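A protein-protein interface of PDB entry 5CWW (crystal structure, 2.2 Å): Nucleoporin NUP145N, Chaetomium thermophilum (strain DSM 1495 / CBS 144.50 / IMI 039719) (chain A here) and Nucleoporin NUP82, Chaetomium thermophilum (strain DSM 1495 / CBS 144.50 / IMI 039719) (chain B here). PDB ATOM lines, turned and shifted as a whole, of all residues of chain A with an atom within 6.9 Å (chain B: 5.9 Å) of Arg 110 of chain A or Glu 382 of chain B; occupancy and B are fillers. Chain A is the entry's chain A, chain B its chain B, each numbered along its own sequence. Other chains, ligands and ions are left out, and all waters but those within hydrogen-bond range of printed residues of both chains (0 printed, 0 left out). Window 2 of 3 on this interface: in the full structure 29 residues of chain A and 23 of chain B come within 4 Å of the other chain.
Among the printed residues, merely in contact across the chains: Arg 110 of chain A with Val 387 of chain B (3.9 Å).
Of chain B, only Glu 382, Asp 384 and Val 387 come within 4 Å of Arg 110 of chain A.
Glu 382 of chain B touches just one residue of chain A: Arg 110 (3.5 Å).
Of the printed residues of chain A, Ser 278 of chain B touches Arg 114.
Of the printed residues of chain A, Asp 384 of chain B touches Arg 106 and Arg 110.
Of the printed residues of chain A, Val 387 of chain B touches Arg 110 (3.9 Å).
The nearest residue of chain B that does not touch Arg 110 of chain A is Gln 383 of chain B (4.1 Å).
Of the 11 printed residues of chain A, 3 touch a printed residue of chain B.
Hydrophobic or aromatic side chains of chain B within 4 Å of the printed part of chain A: Val 387.
Among the printed residues, Asp or Glu carboxylates within 4 Å of a Lys or Arg side-chain nitrogen of the other chain: Arg 106 of chain A with Asp 384 of chain B and Arg 110 of chain A with Asp 384 of chain B.
The guanidinium group (NH2) of Arg 106 of chain A is in salt-bridge range of the side-chain carboxylate (OD2) of Asp 384 of chain B (3.0 Å).
NH2 of Arg 110 of chain A lies within hydrogen-bond range of O of Glu 382 of chain B.
The guanidinium group (NE) of Arg 110 of chain A lies within salt-bridge range of the side-chain carboxylate (OD1) of Asp 384 of chain B (2.7 Å).
The backbone carbonyl oxygen (O) of Ser 278 of chain B sits at hydrogen-bond distance from the guanidinium group (NH2) of Arg 114 of chain A (3.2 Å).
NH1 of Arg 106 of chain A lies within salt-bridge range of OE2 of Glu 109 of chain A, 3.6 Å away.
OE2 of Glu 113 of chain A lies within salt-bridge range of NH1 of Arg 106 of chain A (2.7 Å).
OE2 of Glu 382 of chain B lies within hydrogen-bond range of ND2 of Asn 378 of chain B (3.2 Å).
OE1 of Glu 382 of chain B is in salt-bridge range of NZ of Lys 438 of chain B.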
ATOM      1  N   GLY A 105     -22.621 -22.553  -2.237  1.00  0.00           N
ATOM      2  CA  GLY A 105     -22.574 -22.690  -0.794  1.00  0.00           C
ATOM      3  C   GLY A 105     -22.685 -24.139  -0.367  1.00  0.00           C
ATOM      4  O   GLY A 105     -22.223 -25.039  -1.072  1.00  0.00           O
ATOM      5  N   ARG A 106     -23.306 -24.368   0.784  1.00  0.00           N
ATOM      6  CA  ARG A 106     -23.427 -25.715   1.329  1.00  0.00           C
ATOM      7  C   ARG A 106     -24.253 -26.620   0.417  1.00  0.00           C
ATOM      8  O   ARG A 106     -23.994 -27.820   0.327  1.00  0.00           O
ATOM      9  CB  ARG A 106     -24.045 -25.668   2.732  1.00  0.00           C
ATOM     10  CG  ARG A 106     -24.339 -27.040   3.339  1.00  0.00           C
ATOM     11  CD  ARG A 106     -23.103 -27.930   3.402  1.00  0.00           C
ATOM     12  NE  ARG A 106     -23.440 -29.294   3.801  1.00  0.00           N
ATOM     13  CZ  ARG A 106     -22.628 -30.340   3.673  1.00  0.00           C
ATOM     14  NH1 ARG A 106     -21.418 -30.193   3.147  1.00  0.00           N
ATOM     15  NH2 ARG A 106     -23.031 -31.541   4.064  1.00  0.00           N
ATOM     16  N   ARG A 107     -25.241 -26.042  -0.259  1.00  0.00           N
ATOM     17  CA  ARG A 107     -26.143 -26.811  -1.112  1.00  0.00           C
ATOM     18  C   ARG A 107     -25.395 -27.470  -2.270  1.00  0.00           C
ATOM     19  O   ARG A 107     -25.710 -28.593  -2.664  1.00  0.00           O
ATOM     20  CB  ARG A 107     -27.263 -25.917  -1.648  1.00  0.00           C
ATOM     21  CG  ARG A 107     -28.173 -25.362  -0.563  1.00  0.00           C
ATOM     22  CD  ARG A 107     -29.369 -24.622  -1.145  1.00  0.00           C
ATOM     23  NE  ARG A 107     -28.972 -23.481  -1.965  1.00  0.00           N
ATOM     24  CZ  ARG A 107     -29.826 -22.677  -2.592  1.00  0.00           C
ATOM     25  NH1 ARG A 107     -31.134 -22.883  -2.499  1.00  0.00           N
ATOM     26  NH2 ARG A 107     -29.371 -21.663  -3.317  1.00  0.00           N
ATOM     27  N   LEU A 108     -24.404 -26.769  -2.811  1.00  0.00           N
ATOM     28  CA  LEU A 108     -23.641 -27.276  -3.944  1.00  0.00           C
ATOM     29  C   LEU A 108     -22.671 -28.374  -3.520  1.00  0.00           C
ATOM     30  O   LEU A 108     -22.513 -29.372  -4.225  1.00  0.00           O
ATOM     31  CB  LEU A 108     -22.874 -26.141  -4.627  1.00  0.00           C
ATOM     32  CG  LEU A 108     -22.002 -26.538  -5.823  1.00  0.00           C
ATOM     33  CD1 LEU A 108     -22.831 -27.190  -6.920  1.00  0.00           C
ATOM     34  CD2 LEU A 108     -21.260 -25.328  -6.363  1.00  0.00           C
ATOM     35  N   GLU A 109     -22.012 -28.195  -2.380  1.00  0.00           N
ATOM     36  CA  GLU A 109     -21.063 -29.198  -1.910  1.00  0.00           C
ATOM     37  C   GLU A 109     -21.812 -30.415  -1.378  1.00  0.00           C
ATOM     38  O   GLU A 109     -21.300 -31.532  -1.417  1.00  0.00           O
ATOM     39  CB  GLU A 109     -20.132 -28.622  -0.839  1.00  0.00           C
ATOM     40  CG  GLU A 109     -20.827 -28.095   0.398  1.00  0.00           C
ATOM     41  CD  GLU A 109     -19.857 -27.457   1.380  1.00  0.00           C
ATOM     42  OE1 GLU A 109     -18.633 -27.528   1.140  1.00  0.00           O
ATOM     43  OE2 GLU A 109     -20.317 -26.885   2.391  1.00  0.00           O
ATOM     44  N   ARG A 110     -23.033 -30.201  -0.898  1.00  0.00           N
ATOM     45  CA  ARG A 110     -23.883 -31.310  -0.483  1.00  0.00           C
ATOM     46  C   ARG A 110     -24.215 -32.168  -1.708  1.00  0.00           C
ATOM     47  O   ARG A 110     -24.237 -33.397  -1.635  1.00  0.00           O
ATOM     48  CB  ARG A 110     -25.156 -30.790   0.195  1.00  0.00           C
ATOM     49  CG  ARG A 110     -26.020 -31.877   0.817  1.00  0.00           C
ATOM     50  CD  ARG A 110     -27.319 -31.325   1.401  1.00  0.00           C
ATOM     51  NE  ARG A 110     -27.110 -30.585   2.647  1.00  0.00           N
ATOM     52  CZ  ARG A 110     -27.315 -29.279   2.819  1.00  0.00           C
ATOM     53  NH1 ARG A 110     -27.749 -28.512   1.828  1.00  0.00           N
ATOM     54  NH2 ARG A 110     -27.087 -28.733   4.005  1.00  0.00           N
ATOM     55  N   HIS A 111     -24.458 -31.507  -2.835  1.00  0.00           N
ATOM     56  CA  HIS A 111     -24.776 -32.193  -4.084  1.00  0.00           C
ATOM     57  C   HIS A 111     -23.618 -33.064  -4.565  1.00  0.00           C
ATOM     58  O   HIS A 111     -23.825 -34.179  -5.038  1.00  0.00           O
ATOM     59  CB  HIS A 111     -25.142 -31.179  -5.165  1.00  0.00           C
ATOM     60  CG  HIS A 111     -25.409 -31.790  -6.506  1.00  0.00           C
ATOM     61  ND1 HIS A 111     -26.507 -32.584  -6.758  1.00  0.00           N
ATOM     62  CD2 HIS A 111     -24.722 -31.716  -7.669  1.00  0.00           C
ATOM     63  CE1 HIS A 111     -26.484 -32.975  -8.019  1.00  0.00           C
ATOM     64  NE2 HIS A 111     -25.411 -32.462  -8.595  1.00  0.00           N
ATOM     65  N   ILE A 112     -22.400 -32.542  -4.449  1.00  0.00           N
ATOM     66  CA  ILE A 112     -21.208 -33.287  -4.840  1.00  0.00           C
ATOM     67  C   ILE A 112     -21.007 -34.495  -3.927  1.00  0.00           C
ATOM     68  O   ILE A 112     -20.525 -35.538  -4.367  1.00  0.00           O
ATOM     69  CB  ILE A 112     -19.950 -32.389  -4.808  1.00  0.00           C
ATOM     70  CG1 ILE A 112     -20.103 -31.242  -5.811  1.00  0.00           C
ATOM     71  CG2 ILE A 112     -18.692 -33.192  -5.132  1.00  0.00           C
ATOM     72  CD1 ILE A 112     -19.054 -30.152  -5.676  1.00  0.00           C
ATOM     73  N   GLU A 113     -21.379 -34.352  -2.659  1.00  0.00           N
ATOM     74  CA  GLU A 113     -21.310 -35.462  -1.715  1.00  0.00           C
ATOM     75  C   GLU A 113     -22.261 -36.577  -2.139  1.00  0.00           C
ATOM     76  O   GLU A 113     -21.934 -37.759  -2.041  1.00  0.00           O
ATOM     77  CB  GLU A 113     -21.646 -34.987  -0.297  1.00  0.00           C
ATOM     78  CG  GLU A 113     -20.584 -34.096   0.335  1.00  0.00           C
ATOM     79  CD  GLU A 113     -21.086 -33.350   1.562  1.00  0.00           C
ATOM     80  OE1 GLU A 113     -22.178 -33.685   2.068  1.00  0.00           O
ATOM     81  OE2 GLU A 113     -20.386 -32.421   2.021  1.00  0.00           O
ATOM     82  N   ARG A 114     -23.436 -36.189  -2.625  1.00  0.00           N
ATOM     83  CA  ARG A 114     -24.464 -37.149  -3.010  1.00  0.00           C
ATOM     84  C   ARG A 114     -24.093 -37.875  -4.302  1.00  0.00           C
ATOM     85  O   ARG A 114     -24.422 -39.048  -4.476  1.00  0.00           O
ATOM     86  CB  ARG A 114     -25.812 -36.444  -3.168  1.00  0.00           C
ATOM     87  CG  ARG A 114     -26.380 -35.900  -1.859  1.00  0.00           C
ATOM     88  CD  ARG A 114     -27.403 -34.800  -2.109  1.00  0.00           C
ATOM     89  NE  ARG A 114     -28.175 -34.462  -0.917  1.00  0.00           N
ATOM     90  CZ  ARG A 114     -29.087 -33.496  -0.868  1.00  0.00           C
ATOM     91  NH1 ARG A 114     -29.341 -32.764  -1.945  1.00  0.00           N
ATOM     92  NH2 ARG A 114     -29.746 -33.258   0.258  1.00  0.00           N
ATOM     93  N   LEU A 115     -23.408 -37.177  -5.202  1.00  0.00           N
ATOM     94  CA  LEU A 115     -22.941 -37.783  -6.446  1.00  0.00           C
ATOM     95  C   LEU A 115     -21.926 -38.883  -6.154  1.00  0.00           C
ATOM     96  O   LEU A 115     -21.956 -39.947  -6.770  1.00  0.00           O
ATOM     97  CB  LEU A 115     -22.324 -36.727  -7.367  1.00  0.00           C
ATOM     98  CG  LEU A 115     -23.291 -35.717  -7.992  1.00  0.00           C
ATOM     99  CD1 LEU A 115     -22.525 -34.576  -8.644  1.00  0.00           C
ATOM    100  CD2 LEU A 115     -24.198 -36.395  -9.007  1.00  0.00           C
ATOM    101  N   SER B 278     -34.124 -35.272  -0.802  1.00  0.00           N
ATOM    102  CA  SER B 278     -33.104 -34.267  -1.072  1.00  0.00           C
ATOM    103  C   SER B 278     -33.481 -32.915  -0.470  1.00  0.00           C
ATOM    104  O   SER B 278     -32.628 -32.045  -0.317  1.00  0.00           O
ATOM    105  CB  SER B 278     -32.889 -34.118  -2.579  1.00  0.00           C
ATOM    106  OG  SER B 278     -34.050 -33.598  -3.202  1.00  0.00           O
ATOM    107  N   ASN B 378     -36.531 -18.735   3.664  1.00  0.00           N
ATOM    108  CA  ASN B 378     -36.075 -19.991   4.246  1.00  0.00           C
ATOM    109  C   ASN B 378     -34.974 -19.736   5.274  1.00  0.00           C
ATOM    110  O   ASN B 378     -34.143 -18.850   5.081  1.00  0.00           O
ATOM    111  CB  ASN B 378     -35.569 -20.928   3.149  1.00  0.00           C
ATOM    112  CG  ASN B 378     -35.289 -22.326   3.659  1.00  0.00           C
ATOM    113  OD1 ASN B 378     -36.212 -23.090   3.936  1.00  0.00           O
ATOM    114  ND2 ASN B 378     -34.011 -22.674   3.770  1.00  0.00           N
ATOM    115  N   PRO B 379     -34.969 -20.500   6.380  1.00  0.00           N
ATOM    116  CA  PRO B 379     -33.854 -20.375   7.326  1.00  0.00           C
ATOM    117  C   PRO B 379     -32.512 -20.652   6.659  1.00  0.00           C
ATOM    118  O   PRO B 379     -32.409 -21.574   5.851  1.00  0.00           O
ATOM    119  CB  PRO B 379     -34.167 -21.435   8.387  1.00  0.00           C
ATOM    120  CG  PRO B 379     -35.632 -21.650   8.294  1.00  0.00           C
ATOM    121  CD  PRO B 379     -35.986 -21.454   6.853  1.00  0.00           C
ATOM    122  N   GLU B 380     -31.502 -19.854   6.986  1.00  0.00           N
ATOM    123  CA  GLU B 380     -30.183 -20.023   6.394  1.00  0.00           C
ATOM    124  C   GLU B 380     -29.330 -20.944   7.261  1.00  0.00           C
ATOM    125  O   GLU B 380     -29.582 -21.092   8.458  1.00  0.00           O
ATOM    126  CB  GLU B 380     -29.495 -18.666   6.213  1.00  0.00           C
ATOM    127  CG  GLU B 380     -29.387 -17.835   7.482  1.00  0.00           C
ATOM    128  CD  GLU B 380     -28.759 -16.475   7.236  1.00  0.00           C
ATOM    129  OE1 GLU B 380     -28.523 -16.130   6.059  1.00  0.00           O
ATOM    130  OE2 GLU B 380     -28.503 -15.749   8.221  1.00  0.00           O
ATOM    131  N   ASP B 381     -28.337 -21.572   6.638  1.00  0.00           N
ATOM    132  CA  ASP B 381     -27.421 -22.478   7.326  1.00  0.00           C
ATOM    133  C   ASP B 381     -28.146 -23.670   7.948  1.00  0.00           C
ATOM    134  O   ASP B 381     -27.858 -24.061   9.079  1.00  0.00           O
ATOM    135  CB  ASP B 381     -26.630 -21.727   8.402  1.00  0.00           C
ATOM    136  CG  ASP B 381     -25.836 -20.566   7.836  1.00  0.00           C
ATOM    137  OD1 ASP B 381     -25.482 -20.617   6.640  1.00  0.00           O
ATOM    138  OD2 ASP B 381     -25.565 -19.606   8.586  1.00  0.00           O
ATOM    139  N   GLU B 382     -29.082 -24.246   7.202  1.00  0.00           N
ATOM    140  CA  GLU B 382     -29.759 -25.462   7.635  1.00  0.00           C
ATOM    141  C   GLU B 382     -28.791 -26.641   7.596  1.00  0.00           C
ATOM    142  O   GLU B 382     -27.968 -26.745   6.686  1.00  0.00           O
ATOM    143  CB  GLU B 382     -30.976 -25.757   6.755  1.00  0.00           C
ATOM    144  CG  GLU B 382     -32.167 -24.846   7.001  1.00  0.00           C
ATOM    145  CD  GLU B 382     -33.359 -25.197   6.127  1.00  0.00           C
ATOM    146  OE1 GLU B 382     -34.498 -25.181   6.639  1.00  0.00           O
ATOM    147  OE2 GLU B 382     -33.157 -25.486   4.928  1.00  0.00           O
ATOM    148  N   GLN B 383     -28.895 -27.526   8.583  1.00  0.00           N
ATOM    149  CA  GLN B 383     -28.070 -28.728   8.622  1.00  0.00           C
ATOM    150  C   GLN B 383     -28.623 -29.785   7.671  1.00  0.00           C
ATOM    151  O   GLN B 383     -29.716 -29.630   7.130  1.00  0.00           O
ATOM    152  CB  GLN B 383     -27.998 -29.279  10.046  1.00  0.00           C
ATOM    153  CG  GLN B 383     -27.377 -28.315  11.042  1.00  0.00           C
ATOM    154  CD  GLN B 383     -25.952 -27.944  10.677  1.00  0.00           C
ATOM    155  OE1 GLN B 383     -25.061 -28.793  10.664  1.00  0.00           O
ATOM    156  NE2 GLN B 383     -25.733 -26.672  10.368  1.00  0.00           N
ATOM    157  N   ASP B 384     -27.865 -30.859   7.471  1.00  0.00           N
ATOM    158  CA  ASP B 384     -28.267 -31.913   6.545  1.00  0.00           C
ATOM    159  C   ASP B 384     -29.585 -32.556   6.971  1.00  0.00           C
ATOM    160  O   ASP B 384     -30.460 -32.793   6.140  1.00  0.00           O
ATOM    161  CB  ASP B 384     -27.174 -32.982   6.431  1.00  0.00           C
ATOM    162  CG  ASP B 384     -25.938 -32.485   5.691  1.00  0.00           C
ATOM    163  OD1 ASP B 384     -26.044 -31.497   4.933  1.00  0.00           O
ATOM    164  OD2 ASP B 384     -24.859 -33.091   5.862  1.00  0.00           O
ATOM    165  N   GLU B 386     -31.876 -31.251   8.542  1.00  0.00           N
ATOM    166  CA  GLU B 386     -32.935 -30.246   8.499  1.00  0.00           C
ATOM    167  C   GLU B 386     -33.425 -30.048   7.067  1.00  0.00           C
ATOM    168  O   GLU B 386     -34.611 -29.816   6.834  1.00  0.00           O
ATOM    169  CB  GLU B 386     -32.443 -28.917   9.081  1.00  0.00           C
ATOM    170  CG  GLU B 386     -32.227 -28.947  10.589  1.00  0.00           C
ATOM    171  CD  GLU B 386     -31.563 -27.689  11.122  1.00  0.00           C
ATOM    172  OE1 GLU B 386     -30.860 -27.006  10.350  1.00  0.00           O
ATOM    173  OE2 GLU B 386     -31.743 -27.386  12.321  1.00  0.00           O
ATOM    174  N   VAL B 387     -32.509 -30.145   6.109  1.00  0.00           N
ATOM    175  CA  VAL B 387     -32.863 -30.007   4.701  1.00  0.00           C
ATOM    176  C   VAL B 387     -33.575 -31.270   4.231  1.00  0.00           C
ATOM    177  O   VAL B 387     -34.574 -31.204   3.515  1.00  0.00           O
ATOM    178  CB  VAL B 387     -31.615 -29.750   3.822  1.00  0.00           C
ATOM    179  CG1 VAL B 387     -31.977 -29.743   2.339  1.00  0.00           C
ATOM    180  CG2 VAL B 387     -30.960 -28.435   4.207  1.00  0.00           C
ATOM    181  N   GLN B 436     -37.615 -31.401  12.507  1.00  0.00           N
ATOM    182  CA  GLN B 436     -37.933 -30.011  12.208  1.00  0.00           C
ATOM    183  C   GLN B 436     -39.203 -29.935  11.373  1.00  0.00           C
ATOM    184  O   GLN B 436     -39.376 -30.699  10.422  1.00  0.00           O
ATOM    185  CB  GLN B 436     -36.775 -29.334  11.467  1.00  0.00           C
ATOM    186  CG  GLN B 436     -37.045 -27.887  11.047  1.00  0.00           C
ATOM    187  CD  GLN B 436     -36.128 -27.419   9.931  1.00  0.00           C
ATOM    188  OE1 GLN B 436     -36.397 -27.653   8.747  1.00  0.00           O
ATOM    189  NE2 GLN B 436     -35.043 -26.752  10.301  1.00  0.00           N
ATOM    190  N   LYS B 438     -41.655 -27.288   9.107  1.00  0.00           N
ATOM    191  CA  LYS B 438     -41.672 -26.027   8.386  1.00  0.00           C
ATOM    192  C   LYS B 438     -43.069 -25.772   7.839  1.00  0.00           C
ATOM    193  O   LYS B 438     -43.629 -26.609   7.132  1.00  0.00           O
ATOM    194  CB  LYS B 438     -40.639 -26.044   7.260  1.00  0.00           C
ATOM    195  CG  LYS B 438     -40.356 -24.680   6.657  1.00  0.00           C
ATOM    196  CD  LYS B 438     -39.218 -24.736   5.646  1.00  0.00           C
ATOM    197  CE  LYS B 438     -37.871 -24.971   6.321  1.00  0.00           C
ATOM    198  NZ  LYS B 438     -36.791 -25.222   5.334  1.00  0.00           N
ATOM    199  N   THR B 475     -40.699 -22.055  11.221  1.00  0.00           N
ATOM    200  CA  THR B 475     -39.899 -23.268  11.297  1.00  0.00           C
ATOM    201  C   THR B 475     -39.578 -23.547  12.757  1.00  0.00           C
ATOM    202  O   THR B 475     -39.108 -22.658  13.464  1.00  0.00           O
ATOM    203  CB  THR B 475     -38.583 -23.141  10.500  1.00  0.00           C
ATOM    204  OG1 THR B 475     -38.862 -22.691   9.168  1.00  0.00           O
ATOM    205  CG2 THR B 475     -37.848 -24.476  10.443  1.00  0.00           C
